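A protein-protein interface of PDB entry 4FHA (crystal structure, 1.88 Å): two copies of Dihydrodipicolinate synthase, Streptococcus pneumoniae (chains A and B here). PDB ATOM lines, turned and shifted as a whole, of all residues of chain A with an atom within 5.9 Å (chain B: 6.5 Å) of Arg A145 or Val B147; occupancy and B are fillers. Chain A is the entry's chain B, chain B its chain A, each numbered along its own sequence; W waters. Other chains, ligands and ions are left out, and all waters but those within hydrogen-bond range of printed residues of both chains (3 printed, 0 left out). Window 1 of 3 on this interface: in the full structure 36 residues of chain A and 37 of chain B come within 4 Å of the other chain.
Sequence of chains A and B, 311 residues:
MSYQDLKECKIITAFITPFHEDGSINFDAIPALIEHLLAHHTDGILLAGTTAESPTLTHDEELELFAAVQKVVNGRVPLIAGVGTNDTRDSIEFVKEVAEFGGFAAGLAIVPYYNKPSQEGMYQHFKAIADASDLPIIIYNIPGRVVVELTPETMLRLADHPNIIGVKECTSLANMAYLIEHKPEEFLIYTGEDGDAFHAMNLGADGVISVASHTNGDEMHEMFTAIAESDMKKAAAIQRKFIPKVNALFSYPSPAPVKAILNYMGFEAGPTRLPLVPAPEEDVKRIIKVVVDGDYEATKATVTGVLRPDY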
ATOM      1  N   THR A  50      -7.393   1.329 -10.995  1.00  0.00           N
ATOM      2  CA  THR A  50      -6.513   1.835  -9.939  1.00  0.00           C
ATOM      3  C   THR A  50      -7.329   2.248  -8.721  1.00  0.00           C
ATOM      4  O   THR A  50      -7.038   1.832  -7.598  1.00  0.00           O
ATOM      5  CB  THR A  50      -5.676   3.045 -10.412  1.00  0.00           C
ATOM      6  OG1 THR A  50      -5.128   2.776 -11.706  1.00  0.00           O
ATOM      7  CG2 THR A  50      -4.544   3.327  -9.431  1.00  0.00           C
ATOM      8  N   ILE A 110      -3.351  -1.892 -18.260  1.00  0.00           N
ATOM      9  CA  ILE A 110      -2.403  -0.819 -17.970  1.00  0.00           C
ATOM     10  C   ILE A 110      -1.030  -1.118 -18.566  1.00  0.00           C
ATOM     11  O   ILE A 110      -0.624  -2.279 -18.659  1.00  0.00           O
ATOM     12  CB  ILE A 110      -2.286  -0.579 -16.443  1.00  0.00           C
ATOM     13  CG1 ILE A 110      -1.484   0.695 -16.146  1.00  0.00           C
ATOM     14  CG2 ILE A 110      -1.723  -1.808 -15.733  1.00  0.00           C
ATOM     15  CD1 ILE A 110      -1.610   1.181 -14.722  1.00  0.00           C
ATOM     16  N   TYR A 113       3.775  -2.013 -14.962  1.00  0.00           N
ATOM     17  CA  TYR A 113       4.435  -1.234 -13.912  1.00  0.00           C
ATOM     18  C   TYR A 113       5.628  -1.993 -13.354  1.00  0.00           C
ATOM     19  O   TYR A 113       5.686  -3.223 -13.446  1.00  0.00           O
ATOM     20  CB  TYR A 113       3.444  -0.913 -12.781  1.00  0.00           C
ATOM     21  CG  TYR A 113       2.453  -2.024 -12.515  1.00  0.00           C
ATOM     22  CD1 TYR A 113       1.258  -2.098 -13.229  1.00  0.00           C
ATOM     23  CD2 TYR A 113       2.718  -3.010 -11.568  1.00  0.00           C
ATOM     24  CE1 TYR A 113       0.350  -3.118 -13.001  1.00  0.00           C
ATOM     25  CE2 TYR A 113       1.813  -4.036 -11.332  1.00  0.00           C
ATOM     26  CZ  TYR A 113       0.634  -4.084 -12.058  1.00  0.00           C
ATOM     27  OH  TYR A 113      -0.273  -5.096 -11.840  1.00  0.00           O
ATOM     28  N   TYR A 140      -4.335   1.573 -20.961  1.00  0.00           N
ATOM     29  CA  TYR A 140      -4.231   2.531 -19.867  1.00  0.00           C
ATOM     30  C   TYR A 140      -2.786   3.035 -19.780  1.00  0.00           C
ATOM     31  O   TYR A 140      -1.894   2.316 -19.338  1.00  0.00           O
ATOM     32  CB  TYR A 140      -4.691   1.854 -18.571  1.00  0.00           C
ATOM     33  CG  TYR A 140      -4.739   2.704 -17.321  1.00  0.00           C
ATOM     34  CD1 TYR A 140      -4.706   4.098 -17.372  1.00  0.00           C
ATOM     35  CD2 TYR A 140      -4.860   2.096 -16.072  1.00  0.00           C
ATOM     36  CE1 TYR A 140      -4.764   4.857 -16.210  1.00  0.00           C
ATOM     37  CE2 TYR A 140      -4.921   2.844 -14.912  1.00  0.00           C
ATOM     38  CZ  TYR A 140      -4.873   4.219 -14.984  1.00  0.00           C
ATOM     39  OH  TYR A 140      -4.939   4.945 -13.820  1.00  0.00           O
ATOM     40  N   ILE A 142      -0.269   5.637 -18.241  1.00  0.00           N
ATOM     41  CA  ILE A 142      -0.123   6.519 -17.079  1.00  0.00           C
ATOM     42  C   ILE A 142       1.299   6.466 -16.489  1.00  0.00           C
ATOM     43  O   ILE A 142       1.554   5.725 -15.535  1.00  0.00           O
ATOM     44  CB  ILE A 142      -1.225   6.232 -16.013  1.00  0.00           C
ATOM     45  CG1 ILE A 142      -1.130   7.211 -14.832  1.00  0.00           C
ATOM     46  CG2 ILE A 142      -1.188   4.777 -15.564  1.00  0.00           C
ATOM     47  CD1 ILE A 142      -2.398   7.334 -14.010  1.00  0.00           C
ATOM     48  N   PRO A 143       2.235   7.253 -17.070  1.00  0.00           N
ATOM     49  CA  PRO A 143       3.621   7.310 -16.590  1.00  0.00           C
ATOM     50  C   PRO A 143       3.753   7.820 -15.155  1.00  0.00           C
ATOM     51  O   PRO A 143       4.747   7.528 -14.497  1.00  0.00           O
ATOM     52  CB  PRO A 143       4.297   8.287 -17.564  1.00  0.00           C
ATOM     53  CG  PRO A 143       3.179   9.077 -18.156  1.00  0.00           C
ATOM     54  CD  PRO A 143       2.044   8.103 -18.257  1.00  0.00           C
ATOM     55  N   GLY A 144       2.760   8.570 -14.677  1.00  0.00           N
ATOM     56  CA  GLY A 144       2.744   9.047 -13.292  1.00  0.00           C
ATOM     57  C   GLY A 144       2.706   7.922 -12.273  1.00  0.00           C
ATOM     58  O   GLY A 144       3.140   8.096 -11.131  1.00  0.00           O
ATOM     59  N   ARG A 145       2.194   6.765 -12.691  1.00  0.00           N
ATOM     60  CA  ARG A 145       2.101   5.594 -11.824  1.00  0.00           C
ATOM     61  C   ARG A 145       3.021   4.445 -12.221  1.00  0.00           C
ATOM     62  O   ARG A 145       3.392   3.638 -11.374  1.00  0.00           O
ATOM     63  CB  ARG A 145       0.656   5.088 -11.750  1.00  0.00           C
ATOM     64  CG  ARG A 145      -0.247   5.940 -10.879  1.00  0.00           C
ATOM     65  CD  ARG A 145      -1.588   5.266 -10.645  1.00  0.00           C
ATOM     66  NE  ARG A 145      -2.464   6.101  -9.828  1.00  0.00           N
ATOM     67  CZ  ARG A 145      -2.536   6.049  -8.500  1.00  0.00           C
ATOM     68  NH1 ARG A 145      -1.787   5.194  -7.815  1.00  0.00           N
ATOM     69  NH2 ARG A 145      -3.368   6.855  -7.853  1.00  0.00           N
ATOM     70  N   VAL A 146       3.387   4.363 -13.500  1.00  0.00           N
ATOM     71  CA  VAL A 146       4.166   3.213 -13.981  1.00  0.00           C
ATOM     72  C   VAL A 146       5.539   3.584 -14.551  1.00  0.00           C
ATOM     73  O   VAL A 146       6.240   2.724 -15.083  1.00  0.00           O
ATOM     74  CB  VAL A 146       3.374   2.349 -15.003  1.00  0.00           C
ATOM     75  CG1 VAL A 146       2.021   1.935 -14.435  1.00  0.00           C
ATOM     76  CG2 VAL A 146       3.194   3.084 -16.322  1.00  0.00           C
ATOM     77  N   VAL A 147       5.913   4.857 -14.404  1.00  0.00           N
ATOM     78  CA  VAL A 147       7.189   5.429 -14.896  1.00  0.00           C
ATOM     79  C   VAL A 147       7.245   5.516 -16.426  1.00  0.00           C
ATOM     80  O   VAL A 147       7.276   6.612 -16.984  1.00  0.00           O
ATOM     81  CB  VAL A 147       8.453   4.727 -14.331  1.00  0.00           C
ATOM     82  CG1 VAL A 147       9.706   5.497 -14.717  1.00  0.00           C
ATOM     83  CG2 VAL A 147       8.380   4.593 -12.816  1.00  0.00           C
ATOM     84  N   PHE A 250      -6.691  14.103  -4.649  1.00  0.00           N
ATOM     85  CA  PHE A 250      -5.389  13.456  -4.811  1.00  0.00           C
ATOM     86  C   PHE A 250      -4.334  14.030  -3.862  1.00  0.00           C
ATOM     87  O   PHE A 250      -3.135  13.804  -4.048  1.00  0.00           O
ATOM     88  CB  PHE A 250      -4.933  13.536  -6.274  1.00  0.00           C
ATOM     89  CG  PHE A 250      -5.858  12.835  -7.229  1.00  0.00           C
ATOM     90  CD1 PHE A 250      -6.844  13.543  -7.907  1.00  0.00           C
ATOM     91  CD2 PHE A 250      -5.758  11.463  -7.436  1.00  0.00           C
ATOM     92  CE1 PHE A 250      -7.708  12.898  -8.781  1.00  0.00           C
ATOM     93  CE2 PHE A 250      -6.621  10.811  -8.307  1.00  0.00           C
ATOM     94  CZ  PHE A 250      -7.597  11.529  -8.980  1.00  0.00           C
ATOM     95  N   PRO A 253      -2.759   9.800  -1.109  1.00  0.00           N
ATOM     96  CA  PRO A 253      -2.858   8.757  -2.142  1.00  0.00           C
ATOM     97  C   PRO A 253      -4.270   8.209  -2.364  1.00  0.00           C
ATOM     98  O   PRO A 253      -4.871   7.625  -1.456  1.00  0.00           O
ATOM     99  CB  PRO A 253      -1.928   7.664  -1.620  1.00  0.00           C
ATOM    100  CG  PRO A 253      -0.877   8.423  -0.892  1.00  0.00           C
ATOM    101  CD  PRO A 253      -1.590   9.575  -0.237  1.00  0.00           C
ATOM    102  N   SER A 254      -4.779   8.415  -3.576  1.00  0.00           N
ATOM    103  CA  SER A 254      -6.086   7.917  -3.992  1.00  0.00           C
ATOM    104  C   SER A 254      -6.130   6.386  -3.900  1.00  0.00           C
ATOM    105  O   SER A 254      -5.137   5.723  -4.213  1.00  0.00           O
ATOM    106  CB  SER A 254      -6.376   8.382  -5.421  1.00  0.00           C
ATOM    107  OG  SER A 254      -7.738   8.210  -5.762  1.00  0.00           O
ATOM    108  N   PRO B 112       6.160  -0.479  -2.371  1.00  0.00           N
ATOM    109  CA  PRO B 112       5.062  -0.835  -3.280  1.00  0.00           C
ATOM    110  C   PRO B 112       4.960   0.022  -4.542  1.00  0.00           C
ATOM    111  O   PRO B 112       4.994   1.251  -4.474  1.00  0.00           O
ATOM    112  CB  PRO B 112       3.825  -0.652  -2.406  1.00  0.00           C
ATOM    113  CG  PRO B 112       4.316  -1.007  -1.044  1.00  0.00           C
ATOM    114  CD  PRO B 112       5.696  -0.411  -0.973  1.00  0.00           C
ATOM    115  N   TYR B 113       4.826  -0.658  -5.679  1.00  0.00           N
ATOM    116  CA  TYR B 113       4.744  -0.041  -7.003  1.00  0.00           C
ATOM    117  C   TYR B 113       3.295   0.143  -7.442  1.00  0.00           C
ATOM    118  O   TYR B 113       2.392  -0.539  -6.942  1.00  0.00           O
ATOM    119  CB  TYR B 113       5.478  -0.911  -8.038  1.00  0.00           C
ATOM    120  CG  TYR B 113       5.340  -2.399  -7.787  1.00  0.00           C
ATOM    121  CD1 TYR B 113       6.268  -3.075  -6.999  1.00  0.00           C
ATOM    122  CD2 TYR B 113       4.276  -3.125  -8.321  1.00  0.00           C
ATOM    123  CE1 TYR B 113       6.147  -4.430  -6.751  1.00  0.00           C
ATOM    124  CE2 TYR B 113       4.147  -4.486  -8.080  1.00  0.00           C
ATOM    125  CZ  TYR B 113       5.083  -5.129  -7.290  1.00  0.00           C
ATOM    126  OH  TYR B 113       4.973  -6.474  -7.033  1.00  0.00           O
ATOM    127  N   TYR B 114       3.091   1.063  -8.384  1.00  0.00           N
ATOM    128  CA  TYR B 114       1.783   1.336  -8.997  1.00  0.00           C
ATOM    129  C   TYR B 114       0.792   2.081  -8.082  1.00  0.00           C
ATOM    130  O   TYR B 114       0.301   3.144  -8.461  1.00  0.00           O
ATOM    131  CB  TYR B 114       1.186   0.060  -9.621  1.00  0.00           C
ATOM    132  CG  TYR B 114      -0.187   0.204 -10.250  1.00  0.00           C
ATOM    133  CD1 TYR B 114      -0.590   1.392 -10.859  1.00  0.00           C
ATOM    134  CD2 TYR B 114      -1.071  -0.872 -10.266  1.00  0.00           C
ATOM    135  CE1 TYR B 114      -1.847   1.517 -11.429  1.00  0.00           C
ATOM    136  CE2 TYR B 114      -2.328  -0.759 -10.841  1.00  0.00           C
ATOM    137  CZ  TYR B 114      -2.709   0.432 -11.422  1.00  0.00           C
ATOM    138  OH  TYR B 114      -3.955   0.544 -11.997  1.00  0.00           O
ATOM    139  N   ASN B 115       0.507   1.542  -6.894  1.00  0.00           N
ATOM    140  CA  ASN B 115      -0.482   2.166  -5.993  1.00  0.00           C
ATOM    141  C   ASN B 115      -0.002   3.405  -5.218  1.00  0.00           C
ATOM    142  O   ASN B 115      -0.809   4.103  -4.592  1.00  0.00           O
ATOM    143  CB  ASN B 115      -1.159   1.134  -5.063  1.00  0.00           C
ATOM    144  CG  ASN B 115      -0.171   0.224  -4.346  1.00  0.00           C
ATOM    145  OD1 ASN B 115       1.024   0.507  -4.257  1.00  0.00           O
ATOM    146  ND2 ASN B 115      -0.683  -0.880  -3.815  1.00  0.00           N
ATOM    147  N   LYS B 116       1.304   3.670  -5.273  1.00  0.00           N
ATOM    148  CA  LYS B 116       1.905   4.911  -4.749  1.00  0.00           C
ATOM    149  C   LYS B 116       1.493   5.283  -3.313  1.00  0.00           C
ATOM    150  O   LYS B 116       0.918   6.352  -3.090  1.00  0.00           O
ATOM    151  CB  LYS B 116       1.634   6.078  -5.702  1.00  0.00           C
ATOM    152  CG  LYS B 116       2.370   5.992  -7.032  1.00  0.00           C
ATOM    153  CD  LYS B 116       1.913   7.071  -8.000  1.00  0.00           C
ATOM    154  CE  LYS B 116       2.411   8.451  -7.602  1.00  0.00           C
ATOM    155  NZ  LYS B 116       1.900   9.502  -8.524  1.00  0.00           N
ATOM    156  N   ILE B 142      13.514   2.279  -4.401  1.00  0.00           N
ATOM    157  CA  ILE B 142      13.862   2.597  -5.794  1.00  0.00           C
ATOM    158  C   ILE B 142      12.760   3.389  -6.531  1.00  0.00           C
ATOM    159  O   ILE B 142      11.953   2.809  -7.276  1.00  0.00           O
ATOM    160  CB  ILE B 142      14.316   1.320  -6.567  1.00  0.00           C
ATOM    161  CG1 ILE B 142      14.683   1.642  -8.025  1.00  0.00           C
ATOM    162  CG2 ILE B 142      13.269   0.214  -6.469  1.00  0.00           C
ATOM    163  CD1 ILE B 142      15.682   0.676  -8.633  1.00  0.00           C
ATOM    164  N   PRO B 143      12.729   4.725  -6.332  1.00  0.00           N
ATOM    165  CA  PRO B 143      11.738   5.588  -6.981  1.00  0.00           C
ATOM    166  C   PRO B 143      11.816   5.556  -8.507  1.00  0.00           C
ATOM    167  O   PRO B 143      10.841   5.885  -9.174  1.00  0.00           O
ATOM    168  CB  PRO B 143      12.087   6.990  -6.461  1.00  0.00           C
ATOM    169  CG  PRO B 143      13.491   6.888  -5.975  1.00  0.00           C
ATOM    170  CD  PRO B 143      13.616   5.496  -5.442  1.00  0.00           C
ATOM    171  N   GLY B 144      12.968   5.158  -9.043  1.00  0.00           N
ATOM    172  CA  GLY B 144      13.150   5.017 -10.487  1.00  0.00           C
ATOM    173  C   GLY B 144      12.279   3.933 -11.103  1.00  0.00           C
ATOM    174  O   GLY B 144      12.036   3.940 -12.310  1.00  0.00           O
ATOM    175  N   ARG B 145      11.806   3.005 -10.273  1.00  0.00           N
ATOM    176  CA  ARG B 145      10.902   1.948 -10.731  1.00  0.00           C
ATOM    177  C   ARG B 145       9.505   2.046 -10.130  1.00  0.00           C
ATOM    178  O   ARG B 145       8.532   1.624 -10.761  1.00  0.00           O
ATOM    179  CB  ARG B 145      11.484   0.564 -10.450  1.00  0.00           C
ATOM    180  CG  ARG B 145      12.678   0.212 -11.316  1.00  0.00           C
ATOM    181  CD  ARG B 145      12.961  -1.274 -11.272  1.00  0.00           C
ATOM    182  NE  ARG B 145      14.092  -1.631 -12.128  1.00  0.00           N
ATOM    183  CZ  ARG B 145      13.991  -1.977 -13.408  1.00  0.00           C
ATOM    184  NH1 ARG B 145      12.803  -2.025 -14.009  1.00  0.00           N
ATOM    185  NH2 ARG B 145      15.085  -2.283 -14.089  1.00  0.00           N
ATOM    186  N   VAL B 146       9.403   2.598  -8.922  1.00  0.00           N
ATOM    187  CA  VAL B 146       8.124   2.616  -8.195  1.00  0.00           C
ATOM    188  C   VAL B 146       7.532   4.014  -7.962  1.00  0.00           C
ATOM    189  O   VAL B 146       6.528   4.157  -7.258  1.00  0.00           O
ATOM    190  CB  VAL B 146       8.199   1.804  -6.871  1.00  0.00           C
ATOM    191  CG1 VAL B 146       8.698   0.392  -7.132  1.00  0.00           C
ATOM    192  CG2 VAL B 146       9.079   2.498  -5.838  1.00  0.00           C
ATOM    193  N   VAL B 147       8.145   5.028  -8.578  1.00  0.00           N
ATOM    194  CA  VAL B 147       7.727   6.440  -8.494  1.00  0.00           C
ATOM    195  C   VAL B 147       7.952   7.038  -7.098  1.00  0.00           C
ATOM    196  O   VAL B 147       8.717   7.985  -6.941  1.00  0.00           O
ATOM    197  CB  VAL B 147       6.274   6.697  -8.990  1.00  0.00           C
ATOM    198  CG1 VAL B 147       5.974   8.190  -9.031  1.00  0.00           C
ATOM    199  CG2 VAL B 147       6.049   6.084 -10.366  1.00  0.00           C
ATOM    200  N   VAL B 148       7.282   6.478  -6.096  1.00  0.00           N
ATOM    201  CA  VAL B 148       7.391   6.972  -4.726  1.00  0.00           C
ATOM    202  C   VAL B 148       8.667   6.464  -4.056  1.00  0.00           C
ATOM    203  O   VAL B 148       9.313   5.543  -4.553  1.00  0.00           O
ATOM    204  CB  VAL B 148       6.159   6.584  -3.880  1.00  0.00           C
ATOM    205  CG1 VAL B 148       4.927   7.343  -4.354  1.00  0.00           C
ATOM    206  CG2 VAL B 148       5.930   5.076  -3.911  1.00  0.00           C
ATOM    207  N   GLU B 149       9.029   7.075  -2.932  1.00  0.00           N
ATOM    208  CA  GLU B 149      10.205   6.648  -2.181  1.00  0.00           C
ATOM    209  C   GLU B 149      10.065   6.878  -0.685  1.00  0.00           C
ATOM    210  O   GLU B 149       9.441   7.850  -0.248  1.00  0.00           O
ATOM    211  CB  GLU B 149      11.469   7.345  -2.700  1.00  0.00           C
ATOM    212  CG  GLU B 149      11.468   8.859  -2.547  1.00  0.00           C
ATOM    213  CD  GLU B 149      12.657   9.517  -3.218  1.00  0.00           C
ATOM    214  OE1 GLU B 149      13.797   9.301  -2.760  1.00  0.00           O
ATOM    215  OE2 GLU B 149      12.446  10.258  -4.199  1.00  0.00           O
HETATM  216  O   HOH W   1      -3.428   3.835  -5.462  1.00  0.00           O
HETATM  217  O   HOH W   2       6.134   1.240 -12.092  1.00  0.00           O
HETATM  218  O   HOH W   3       5.030   2.333  -9.568  1.00  0.00           O
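Printed residues of chain A that touch a printed residue of chain B: Thr A50, Ile A110, Tyr A113, Tyr A140, Gly A144, Arg A145, Val A147 and Pro A253. Hydrophobic or aromatic side chains of chain A that line the printed part of chain B: Ile A110, Tyr A113, Tyr A140, Val A147 and Pro A253. Among the printed residues, 15 pairs touch across the chains.
OD1 of Asn B115 lies close to O of Tyr B113. The side-chain hydroxyl (OG1) of Thr A50 sits at hydrogen-bond distance from the side-chain hydroxyl (OH) of Tyr A140.
Water W3 lies within hydrogen-bond range of N of Tyr B114 (2.6 Å), O of Arg A145 (2.8 Å) and O of Val B146 (3.3 Å). Water W2 lies within hydrogen-bond range of O of Arg B145 (2.8 Å) and O of Val A146 (3.3 Å). Water W1 lies within hydrogen-bond range of the backbone carbonyl oxygen of Asn B115, the backbone carbonyl oxygen of Ser A254 and the guanidinium group of Arg A145.
Tyr A113 touches its own counterpart, Tyr B113. Gly A144 touches Val B147, and with the chains exchanged Val A147 touches Gly B144. Arg A145 touches Val B147, and with the chains exchanged Val A147 touches Arg B145. Val B147 touches its own counterpart, Val A147. 7 positions are printed for both chains.
Ile A110 touches Tyr B114. Tyr B113 touches Tyr A113 (CD2 to CD2, 3.6 Å). CG of Tyr A113 touches CB of Tyr B114 (3.8 Å). Tyr A140 touches Tyr B114. O of Gly A144 touches CG1 of Val B147, 3.5 Å away. Arg A145 touches Asn B115 (NH1 to O, 3.5 Å). CG of Arg A145 touches CD of Lys B116 (3.8 Å). Arg A145 touches Val B147 (O to CG2, 3.7 Å). O of Arg B145 touches CG2 of Val A147, 3.6 Å away. CB of Pro A253 touches O of Lys B116 (3.5 Å).
Arg A145 touches just these residues of chain B: Tyr B114 (3.0 Å), Asn B115 (3.5 Å), Lys B116 (3.8 Å) and Val B147 (3.7 Å). Val B147 touches three residues of chain A. Of the printed residues of chain A, Gly B144 touches Val A147. Of the printed residues of chain B, Val A147 touches Gly B144 (3.7 Å), Arg B145 (3.6 Å) and Val B147 (3.7 Å). Phe A250 touches none of the printed residues of chain B. Ser A254 touches none of the printed residues of chain B. The nearest printed residue of chain B that does not touch Tyr A140 is Lys B116 (9.2 Å).
The side-chain hydroxyl (OH) of Tyr B114 lies within hydrogen-bond range of the side-chain hydroxyl (OG1) of Thr A50. The backbone carbonyl oxygen (O) of Tyr B114 sits at hydrogen-bond distance from the guanidinium group (NH1) of Arg A145, 3.0 Å away. NZ of Lys B116 sits at hydrogen-bond distance from O of Gly A144 (3.2 Å).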
